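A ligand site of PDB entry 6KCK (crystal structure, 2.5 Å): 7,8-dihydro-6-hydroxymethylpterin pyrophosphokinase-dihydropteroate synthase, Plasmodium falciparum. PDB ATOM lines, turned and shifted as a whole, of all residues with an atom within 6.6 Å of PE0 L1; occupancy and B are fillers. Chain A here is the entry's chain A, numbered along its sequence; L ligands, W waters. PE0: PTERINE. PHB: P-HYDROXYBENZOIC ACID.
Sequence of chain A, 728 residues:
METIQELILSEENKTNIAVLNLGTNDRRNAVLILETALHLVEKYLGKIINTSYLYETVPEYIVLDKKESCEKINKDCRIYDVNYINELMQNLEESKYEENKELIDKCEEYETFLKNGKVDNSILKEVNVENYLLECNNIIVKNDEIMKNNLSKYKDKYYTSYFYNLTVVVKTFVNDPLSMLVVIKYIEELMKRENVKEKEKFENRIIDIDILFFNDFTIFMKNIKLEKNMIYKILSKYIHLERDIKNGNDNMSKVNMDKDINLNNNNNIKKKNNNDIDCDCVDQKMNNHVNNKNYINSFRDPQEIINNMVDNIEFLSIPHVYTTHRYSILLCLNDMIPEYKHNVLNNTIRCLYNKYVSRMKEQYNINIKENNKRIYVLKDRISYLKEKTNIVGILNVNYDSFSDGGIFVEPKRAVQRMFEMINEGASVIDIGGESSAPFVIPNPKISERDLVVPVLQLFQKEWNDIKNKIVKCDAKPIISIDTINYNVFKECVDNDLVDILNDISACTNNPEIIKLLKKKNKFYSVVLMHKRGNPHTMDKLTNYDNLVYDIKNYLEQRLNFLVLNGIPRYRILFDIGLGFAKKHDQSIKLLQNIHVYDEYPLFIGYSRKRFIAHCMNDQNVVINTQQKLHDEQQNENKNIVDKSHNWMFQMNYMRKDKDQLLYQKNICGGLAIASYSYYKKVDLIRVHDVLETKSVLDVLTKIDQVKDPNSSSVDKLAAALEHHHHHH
An oxygen (O4) of PE0 L1 is in hydrogen-bond range of the side-chain amino group (NZ) of Lys 609 (2.5 Å).
N2 of PE0 L1 sits at hydrogen-bond distance from OD2 of Asp 575.
The side-chain carboxylate (OD2) of Asp 482 is in hydrogen-bond range of a nitrogen (N3) of PE0 L1.
The side-chain amide oxygen (OD1) of Asn 502 is in hydrogen-bond range of a nitrogen (N6) of PE0 L1 (2.7 Å).
NH1 of Arg 686 lies close to N4 of PE0 L1, at 3.3 Å.
The side-chain sulfur (SD) of Met 529 lies within hydrogen-bond range of a nitrogen (N2) of PE0 L1, at 3.4 Å.
The backbone carbonyl oxygen of Ser 436 sits close to an oxygen (O4) of PHB L2 (3.3 Å).
The side-chain hydroxyl (OG) of Ser 436 sits at hydrogen-bond distance from an oxygen (O4) of PHB L2, 2.8 Å away.
O4 of PHB L2 lies within hydrogen-bond range of N of Ala 437.
The backbone carbonyl oxygen of Gly 605 sits at hydrogen-bond distance from the side-chain amino group of Lys 609 (2.7 Å).
N of Gly 577 sits at hydrogen-bond distance from OD1 of Asp 575, at 2.9 Å.
The backbone carbonyl oxygen (O) of Leu 528 sits at hydrogen-bond distance from the backbone NH (N) of Asp 575, at 2.9 Å.
The guanidinium group of Arg 686 is in salt-bridge range of the side-chain carboxylate of Asp 482.
The backbone NH (N) of Asp 482 is in hydrogen-bond range of the side-chain carboxylate (OD1) of Asp 430.
ND2 of Asn 502 lies within hydrogen-bond range of OD2 of Asp 430, 3.1 Å away.
N of Met 529 sits at hydrogen-bond distance from O of Asp 503 (3.5 Å).
O of Val 527 lies within hydrogen-bond range of N of Asp 503.
Water W1 lies within hydrogen-bond range of OD1 of Asp 575 (2.6 Å), O4 of PE0 L1 (2.8 Å), N of Leu 578 (3.0 Å) and N of Gly 605 (3.0 Å).
Water W2 lies within hydrogen-bond range of the side-chain carboxylate (OD2) of Asp 482 (2.8 Å), the side-chain hydroxyl (OG) of Ser 436 (2.9 Å) and a nitrogen (N3) of PE0 L1 (3.1 Å).
The backbone carbonyl oxygen of Gly 605 lies close to an oxygen (O4) of PE0 L1, 3.2 Å away.
OG of Ser 436 touches C6 of PE0 L1 (3.98 Å).
CG2 of Ile 504 touches N1 of PE0 L1, 3.7 Å away.
Val 527 touches PE0 L1 (CG1 to N6, 3.8 Å).
Phe 580 touches PE0 L1 (CE1 to N4, 3.6 Å).
Phe 603 touches PE0 L1 (CE1 to N6, 3.6 Å).
Hydrophobic or aromatic side chains that line PE0 L1: Ile 504, Val 527, Met 529, Phe 580 and Phe 603.
Within 4 Å of PE0 L1: Ser 436, Asp 482, Asn 502, Ile 504, Val 527, Met 529, Asp 575, Phe 580, Phe 603, Gly 605, Lys 609 and Arg 686.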
ATOM      1  N   ILE A 394      12.757  -6.950   0.180  1.00  0.00           N
ATOM      2  CA  ILE A 394      12.490  -6.582   1.580  1.00  0.00           C
ATOM      3  C   ILE A 394      12.921  -7.692   2.531  1.00  0.00           C
ATOM      4  O   ILE A 394      12.570  -8.832   2.330  1.00  0.00           O
ATOM      5  CB  ILE A 394      11.002  -6.259   1.796  1.00  0.00           C
ATOM      6  CG1 ILE A 394      10.567  -5.009   0.983  1.00  0.00           C
ATOM      7  CG2 ILE A 394      10.729  -6.039   3.286  1.00  0.00           C
ATOM      8  CD1 ILE A 394       9.060  -4.780   0.904  1.00  0.00           C
ATOM      9  N   ASN A 396      12.332  -8.157   6.358  1.00  0.00           N
ATOM     10  CA  ASN A 396      11.814  -7.732   7.648  1.00  0.00           C
ATOM     11  C   ASN A 396      12.332  -8.697   8.716  1.00  0.00           C
ATOM     12  O   ASN A 396      11.992  -9.882   8.703  1.00  0.00           O
ATOM     13  CB  ASN A 396      10.270  -7.620   7.657  1.00  0.00           C
ATOM     14  CG  ASN A 396       9.728  -6.473   6.754  1.00  0.00           C
ATOM     15  OD1 ASN A 396       8.792  -6.684   5.949  1.00  0.00           O
ATOM     16  ND2 ASN A 396      10.307  -5.257   6.885  1.00  0.00           N
ATOM     17  N   ASP A 430      16.855  -4.419   1.318  1.00  0.00           N
ATOM     18  CA  ASP A 430      16.491  -3.432   2.304  1.00  0.00           C
ATOM     19  C   ASP A 430      16.092  -4.129   3.571  1.00  0.00           C
ATOM     20  O   ASP A 430      15.018  -4.734   3.637  1.00  0.00           O
ATOM     21  CB  ASP A 430      15.297  -2.549   1.842  1.00  0.00           C
ATOM     22  CG  ASP A 430      14.969  -1.398   2.861  1.00  0.00           C
ATOM     23  OD1 ASP A 430      15.932  -0.678   3.264  1.00  0.00           O
ATOM     24  OD2 ASP A 430      13.765  -1.226   3.246  1.00  0.00           O
ATOM     25  N   SER A 436       6.924  -0.198  10.864  1.00  0.00           N
ATOM     26  CA  SER A 436       6.269   1.122  10.795  1.00  0.00           C
ATOM     27  C   SER A 436       4.833   0.916  10.284  1.00  0.00           C
ATOM     28  O   SER A 436       4.136   1.885   9.954  1.00  0.00           O
ATOM     29  CB  SER A 436       7.042   2.071   9.872  1.00  0.00           C
ATOM     30  OG  SER A 436       7.204   1.523   8.541  1.00  0.00           O
ATOM     31  N   ALA A 437       4.405  -0.343  10.225  1.00  0.00           N
ATOM     32  CA  ALA A 437       3.073  -0.721   9.761  1.00  0.00           C
ATOM     33  C   ALA A 437       1.959  -0.124  10.624  1.00  0.00           C
ATOM     34  O   ALA A 437       2.147   0.068  11.818  1.00  0.00           O
ATOM     35  CB  ALA A 437       2.953  -2.253   9.724  1.00  0.00           C
ATOM     36  N   ASP A 482      16.545   0.247   6.526  1.00  0.00           N
ATOM     37  CA  ASP A 482      15.337   0.956   6.884  1.00  0.00           C
ATOM     38  C   ASP A 482      15.352   1.289   8.396  1.00  0.00           C
ATOM     39  O   ASP A 482      14.834   0.516   9.230  1.00  0.00           O
ATOM     40  CB  ASP A 482      14.170   0.049   6.541  1.00  0.00           C
ATOM     41  CG  ASP A 482      12.842   0.728   6.610  1.00  0.00           C
ATOM     42  OD1 ASP A 482      12.696   1.781   7.282  1.00  0.00           O
ATOM     43  OD2 ASP A 482      11.894   0.199   5.982  1.00  0.00           O
ATOM     44  N   ASN A 502      17.799   4.145   4.349  1.00  0.00           N
ATOM     45  CA  ASN A 502      16.424   4.301   3.934  1.00  0.00           C
ATOM     46  C   ASN A 502      15.749   4.973   5.126  1.00  0.00           C
ATOM     47  O   ASN A 502      15.458   4.314   6.154  1.00  0.00           O
ATOM     48  CB  ASN A 502      15.798   2.939   3.570  1.00  0.00           C
ATOM     49  CG  ASN A 502      14.285   3.017   3.270  1.00  0.00           C
ATOM     50  OD1 ASN A 502      13.736   4.114   3.009  1.00  0.00           O
ATOM     51  ND2 ASN A 502      13.605   1.868   3.315  1.00  0.00           N
ATOM     52  N   ASP A 503      15.544   6.291   5.050  1.00  0.00           N
ATOM     53  CA  ASP A 503      14.988   7.025   6.198  1.00  0.00           C
ATOM     54  C   ASP A 503      13.527   7.389   5.938  1.00  0.00           C
ATOM     55  O   ASP A 503      13.231   8.320   5.207  1.00  0.00           O
ATOM     56  CB  ASP A 503      15.816   8.281   6.498  1.00  0.00           C
ATOM     57  CG  ASP A 503      15.493   8.909   7.882  1.00  0.00           C
ATOM     58  OD1 ASP A 503      14.294   9.249   8.202  1.00  0.00           O
ATOM     59  OD2 ASP A 503      16.479   9.122   8.634  1.00  0.00           O
ATOM     60  N   ILE A 504      12.618   6.626   6.496  1.00  0.00           N
ATOM     61  CA  ILE A 504      11.229   6.939   6.320  1.00  0.00           C
ATOM     62  C   ILE A 504      10.785   8.286   6.886  1.00  0.00           C
ATOM     63  O   ILE A 504       9.644   8.682   6.658  1.00  0.00           O
ATOM     64  CB  ILE A 504      10.309   5.839   6.893  1.00  0.00           C
ATOM     65  CG1 ILE A 504      10.526   5.677   8.417  1.00  0.00           C
ATOM     66  CG2 ILE A 504      10.531   4.541   6.113  1.00  0.00           C
ATOM     67  CD1 ILE A 504       9.408   4.907   9.106  1.00  0.00           C
ATOM     68  N   VAL A 527      17.581   7.229   0.793  1.00  0.00           N
ATOM     69  CA  VAL A 527      16.216   7.379   0.391  1.00  0.00           C
ATOM     70  C   VAL A 527      15.502   8.343   1.341  1.00  0.00           C
ATOM     71  O   VAL A 527      15.539   8.192   2.548  1.00  0.00           O
ATOM     72  CB  VAL A 527      15.521   6.002   0.461  1.00  0.00           C
ATOM     73  CG1 VAL A 527      14.067   6.089  -0.013  1.00  0.00           C
ATOM     74  CG2 VAL A 527      16.316   4.986  -0.381  1.00  0.00           C
ATOM     75  N   LEU A 528      14.845   9.343   0.784  1.00  0.00           N
ATOM     76  CA  LEU A 528      14.033  10.242   1.576  1.00  0.00           C
ATOM     77  C   LEU A 528      12.620   9.922   1.239  1.00  0.00           C
ATOM     78  O   LEU A 528      12.214  10.053   0.089  1.00  0.00           O
ATOM     79  CB  LEU A 528      14.294  11.703   1.201  1.00  0.00           C
ATOM     80  CG  LEU A 528      15.711  12.235   1.423  1.00  0.00           C
ATOM     81  CD1 LEU A 528      15.783  13.688   0.986  1.00  0.00           C
ATOM     82  CD2 LEU A 528      16.250  12.057   2.828  1.00  0.00           C
ATOM     83  N   MET A 529      11.873   9.496   2.236  1.00  0.00           N
ATOM     84  CA  MET A 529      10.471   9.164   2.086  1.00  0.00           C
ATOM     85  C   MET A 529       9.595  10.231   2.790  1.00  0.00           C
ATOM     86  O   MET A 529      10.042  10.814   3.812  1.00  0.00           O
ATOM     87  CB  MET A 529      10.189   7.775   2.701  1.00  0.00           C
ATOM     88  CG  MET A 529       8.841   7.222   2.230  1.00  0.00           C
ATOM     89  SD  MET A 529       8.189   5.836   3.153  1.00  0.00           S
ATOM     90  CE  MET A 529       7.551   6.663   4.628  1.00  0.00           C
ATOM     91  N   ASP A 575      10.971   9.181  -2.360  1.00  0.00           N
ATOM     92  CA  ASP A 575       9.927   8.179  -2.160  1.00  0.00           C
ATOM     93  C   ASP A 575       8.680   8.867  -1.633  1.00  0.00           C
ATOM     94  O   ASP A 575       8.724   9.556  -0.613  1.00  0.00           O
ATOM     95  CB  ASP A 575      10.418   7.064  -1.227  1.00  0.00           C
ATOM     96  CG  ASP A 575       9.428   5.907  -1.095  1.00  0.00           C
ATOM     97  OD1 ASP A 575       8.244   6.030  -1.496  1.00  0.00           O
ATOM     98  OD2 ASP A 575       9.847   4.860  -0.533  1.00  0.00           O
ATOM     99  N   GLY A 577       6.213   7.649  -0.318  1.00  0.00           N
ATOM    100  CA  GLY A 577       5.674   6.938   0.813  1.00  0.00           C
ATOM    101  C   GLY A 577       4.235   6.506   0.713  1.00  0.00           C
ATOM    102  O   GLY A 577       3.414   6.981   1.466  1.00  0.00           O
ATOM    103  N   LEU A 578       3.917   5.572  -0.170  1.00  0.00           N
ATOM    104  CA  LEU A 578       2.518   5.123  -0.317  1.00  0.00           C
ATOM    105  C   LEU A 578       2.066   4.541   1.001  1.00  0.00           C
ATOM    106  O   LEU A 578       2.836   3.847   1.675  1.00  0.00           O
ATOM    107  CB  LEU A 578       2.382   4.109  -1.447  1.00  0.00           C
ATOM    108  CG  LEU A 578       2.786   4.607  -2.840  1.00  0.00           C
ATOM    109  CD1 LEU A 578       2.994   3.431  -3.776  1.00  0.00           C
ATOM    110  CD2 LEU A 578       1.759   5.548  -3.441  1.00  0.00           C
ATOM    111  N   PHE A 580       1.575   5.979   3.893  1.00  0.00           N
ATOM    112  CA  PHE A 580       1.978   6.730   5.074  1.00  0.00           C
ATOM    113  C   PHE A 580       1.313   8.088   5.161  1.00  0.00           C
ATOM    114  O   PHE A 580       1.826   9.073   4.566  1.00  0.00           O
ATOM    115  CB  PHE A 580       3.463   6.972   5.098  1.00  0.00           C
ATOM    116  CG  PHE A 580       4.295   5.747   5.368  1.00  0.00           C
ATOM    117  CD1 PHE A 580       4.597   4.835   4.331  1.00  0.00           C
ATOM    118  CD2 PHE A 580       4.844   5.541   6.644  1.00  0.00           C
ATOM    119  CE1 PHE A 580       5.416   3.738   4.572  1.00  0.00           C
ATOM    120  CE2 PHE A 580       5.683   4.453   6.882  1.00  0.00           C
ATOM    121  CZ  PHE A 580       5.984   3.560   5.837  1.00  0.00           C
ATOM    122  N   PHE A 603      12.026   5.982  -5.924  1.00  0.00           N
ATOM    123  CA  PHE A 603      12.049   4.756  -5.188  1.00  0.00           C
ATOM    124  C   PHE A 603      10.633   4.664  -4.637  1.00  0.00           C
ATOM    125  O   PHE A 603      10.189   5.613  -3.991  1.00  0.00           O
ATOM    126  CB  PHE A 603      13.017   4.972  -4.041  1.00  0.00           C
ATOM    127  CG  PHE A 603      13.250   3.785  -3.136  1.00  0.00           C
ATOM    128  CD1 PHE A 603      12.282   3.372  -2.230  1.00  0.00           C
ATOM    129  CD2 PHE A 603      14.507   3.151  -3.114  1.00  0.00           C
ATOM    130  CE1 PHE A 603      12.532   2.318  -1.345  1.00  0.00           C
ATOM    131  CE2 PHE A 603      14.767   2.086  -2.257  1.00  0.00           C
ATOM    132  CZ  PHE A 603      13.770   1.655  -1.366  1.00  0.00           C
ATOM    133  N   ILE A 604       9.910   3.574  -4.904  1.00  0.00           N
ATOM    134  CA  ILE A 604       8.585   3.425  -4.287  1.00  0.00           C
ATOM    135  C   ILE A 604       8.333   2.031  -3.660  1.00  0.00           C
ATOM    136  O   ILE A 604       8.998   1.050  -3.991  1.00  0.00           O
ATOM    137  CB  ILE A 604       7.423   3.797  -5.236  1.00  0.00           C
ATOM    138  CG1 ILE A 604       7.150   2.668  -6.236  1.00  0.00           C
ATOM    139  CG2 ILE A 604       7.656   5.159  -5.916  1.00  0.00           C
ATOM    140  CD1 ILE A 604       6.127   3.035  -7.289  1.00  0.00           C
ATOM    141  N   GLY A 605       7.356   1.965  -2.772  1.00  0.00           N
ATOM    142  CA  GLY A 605       7.118   0.796  -1.953  1.00  0.00           C
ATOM    143  C   GLY A 605       5.642   0.638  -1.871  1.00  0.00           C
ATOM    144  O   GLY A 605       4.956   1.305  -1.106  1.00  0.00           O
ATOM    145  N   TYR A 606       5.112  -0.225  -2.697  1.00  0.00           N
ATOM    146  CA  TYR A 606       3.677  -0.428  -2.705  1.00  0.00           C
ATOM    147  C   TYR A 606       3.394  -1.792  -2.110  1.00  0.00           C
ATOM    148  O   TYR A 606       2.262  -2.087  -1.768  1.00  0.00           O
ATOM    149  CB  TYR A 606       3.182  -0.371  -4.148  1.00  0.00           C
ATOM    150  CG  TYR A 606       3.925  -1.338  -5.053  1.00  0.00           C
ATOM    151  CD1 TYR A 606       3.581  -2.704  -5.091  1.00  0.00           C
ATOM    152  CD2 TYR A 606       4.953  -0.906  -5.889  1.00  0.00           C
ATOM    153  CE1 TYR A 606       4.242  -3.587  -5.912  1.00  0.00           C
ATOM    154  CE2 TYR A 606       5.624  -1.786  -6.732  1.00  0.00           C
ATOM    155  CZ  TYR A 606       5.259  -3.126  -6.728  1.00  0.00           C
ATOM    156  OH  TYR A 606       5.920  -4.023  -7.532  1.00  0.00           O
ATOM    157  N   SER A 607       4.436  -2.610  -1.965  1.00  0.00           N
ATOM    158  CA  SER A 607       4.254  -4.064  -1.743  1.00  0.00           C
ATOM    159  C   SER A 607       3.427  -4.454  -0.513  1.00  0.00           C
ATOM    160  O   SER A 607       3.760  -4.098   0.650  1.00  0.00           O
ATOM    161  CB  SER A 607       5.593  -4.785  -1.730  1.00  0.00           C
ATOM    162  OG  SER A 607       5.389  -6.144  -1.373  1.00  0.00           O
ATOM    163  N   LYS A 609       0.752  -3.415   0.628  1.00  0.00           N
ATOM    164  CA  LYS A 609       0.125  -2.349   1.366  1.00  0.00           C
ATOM    165  C   LYS A 609      -1.384  -2.414   1.165  1.00  0.00           C
ATOM    166  O   LYS A 609      -1.872  -2.970   0.187  1.00  0.00           O
ATOM    167  CB  LYS A 609       0.709  -0.980   0.955  1.00  0.00           C
ATOM    168  CG  LYS A 609       2.196  -0.831   1.316  1.00  0.00           C
ATOM    169  CD  LYS A 609       2.559   0.620   1.569  1.00  0.00           C
ATOM    170  CE  LYS A 609       3.819   0.729   2.395  1.00  0.00           C
ATOM    171  NZ  LYS A 609       4.994   1.257   1.629  1.00  0.00           N
ATOM    172  N   ARG A 686      10.482  -1.400  -4.097  1.00  0.00           N
ATOM    173  CA  ARG A 686      10.704  -2.136  -2.863  1.00  0.00           C
ATOM    174  C   ARG A 686       9.602  -3.213  -2.656  1.00  0.00           C
ATOM    175  O   ARG A 686       8.433  -2.887  -2.427  1.00  0.00           O
ATOM    176  CB  ARG A 686      10.690  -1.142  -1.716  1.00  0.00           C
ATOM    177  CG  ARG A 686      10.950  -1.763  -0.355  1.00  0.00           C
ATOM    178  CD  ARG A 686      10.924  -0.680   0.714  1.00  0.00           C
ATOM    179  NE  ARG A 686      11.212  -1.247   2.021  1.00  0.00           N
ATOM    180  CZ  ARG A 686      10.288  -1.788   2.816  1.00  0.00           C
ATOM    181  NH1 ARG A 686       8.988  -1.838   2.449  1.00  0.00           N
ATOM    182  NH2 ARG A 686      10.683  -2.293   3.971  1.00  0.00           N
HETATM  183  C1  PE0 L   1       8.258   1.642   2.857  1.00  0.00           C
HETATM  184  C4  PE0 L   1       8.163   2.476   1.672  1.00  0.00           C
HETATM  185  O4  PE0 L   1       7.101   2.491   1.014  1.00  0.00           O
HETATM  186  N2  PE0 L   1       9.244   3.196   1.325  1.00  0.00           N
HETATM  187  C3  PE0 L   1      10.396   3.183   2.037  1.00  0.00           C
HETATM  188  N6  PE0 L   1      11.395   3.991   1.589  1.00  0.00           N
HETATM  189  N1  PE0 L   1      10.559   2.407   3.146  1.00  0.00           N
HETATM  190  C2  PE0 L   1       9.540   1.643   3.597  1.00  0.00           C
HETATM  191  N3  PE0 L   1       9.623   0.859   4.719  1.00  0.00           N
HETATM  192  C6  PE0 L   1       8.563   0.102   5.081  1.00  0.00           C
HETATM  193  C5  PE0 L   1       7.340   0.126   4.375  1.00  0.00           C
HETATM  194  N4  PE0 L   1       7.218   0.877   3.255  1.00  0.00           N
HETATM  195  C1' PHB L   2       0.001   0.032   4.612  1.00  0.00           C
HETATM  196  O1' PHB L   2      -0.409  -1.139   4.336  1.00  0.00           O
HETATM  197  O2' PHB L   2      -0.677   1.067   4.396  1.00  0.00           O
HETATM  198  C1  PHB L   2       1.339   0.182   5.262  1.00  0.00           C
HETATM  199  C2  PHB L   2       1.818   1.425   5.607  1.00  0.00           C
HETATM  200  C3  PHB L   2       3.066   1.539   6.227  1.00  0.00           C
HETATM  201  C4  PHB L   2       3.807   0.384   6.490  1.00  0.00           C
HETATM  202  C5  PHB L   2       3.309  -0.881   6.143  1.00  0.00           C
HETATM  203  C6  PHB L   2       2.079  -0.960   5.531  1.00  0.00           C
HETATM  204  O4  PHB L   2       5.037   0.472   7.099  1.00  0.00           O
HETATM  205  O   HOH W   1       6.431   4.231  -1.055  1.00  0.00           O
HETATM  206  O   HOH W   2      10.015   1.060   7.821  1.00  0.00           O
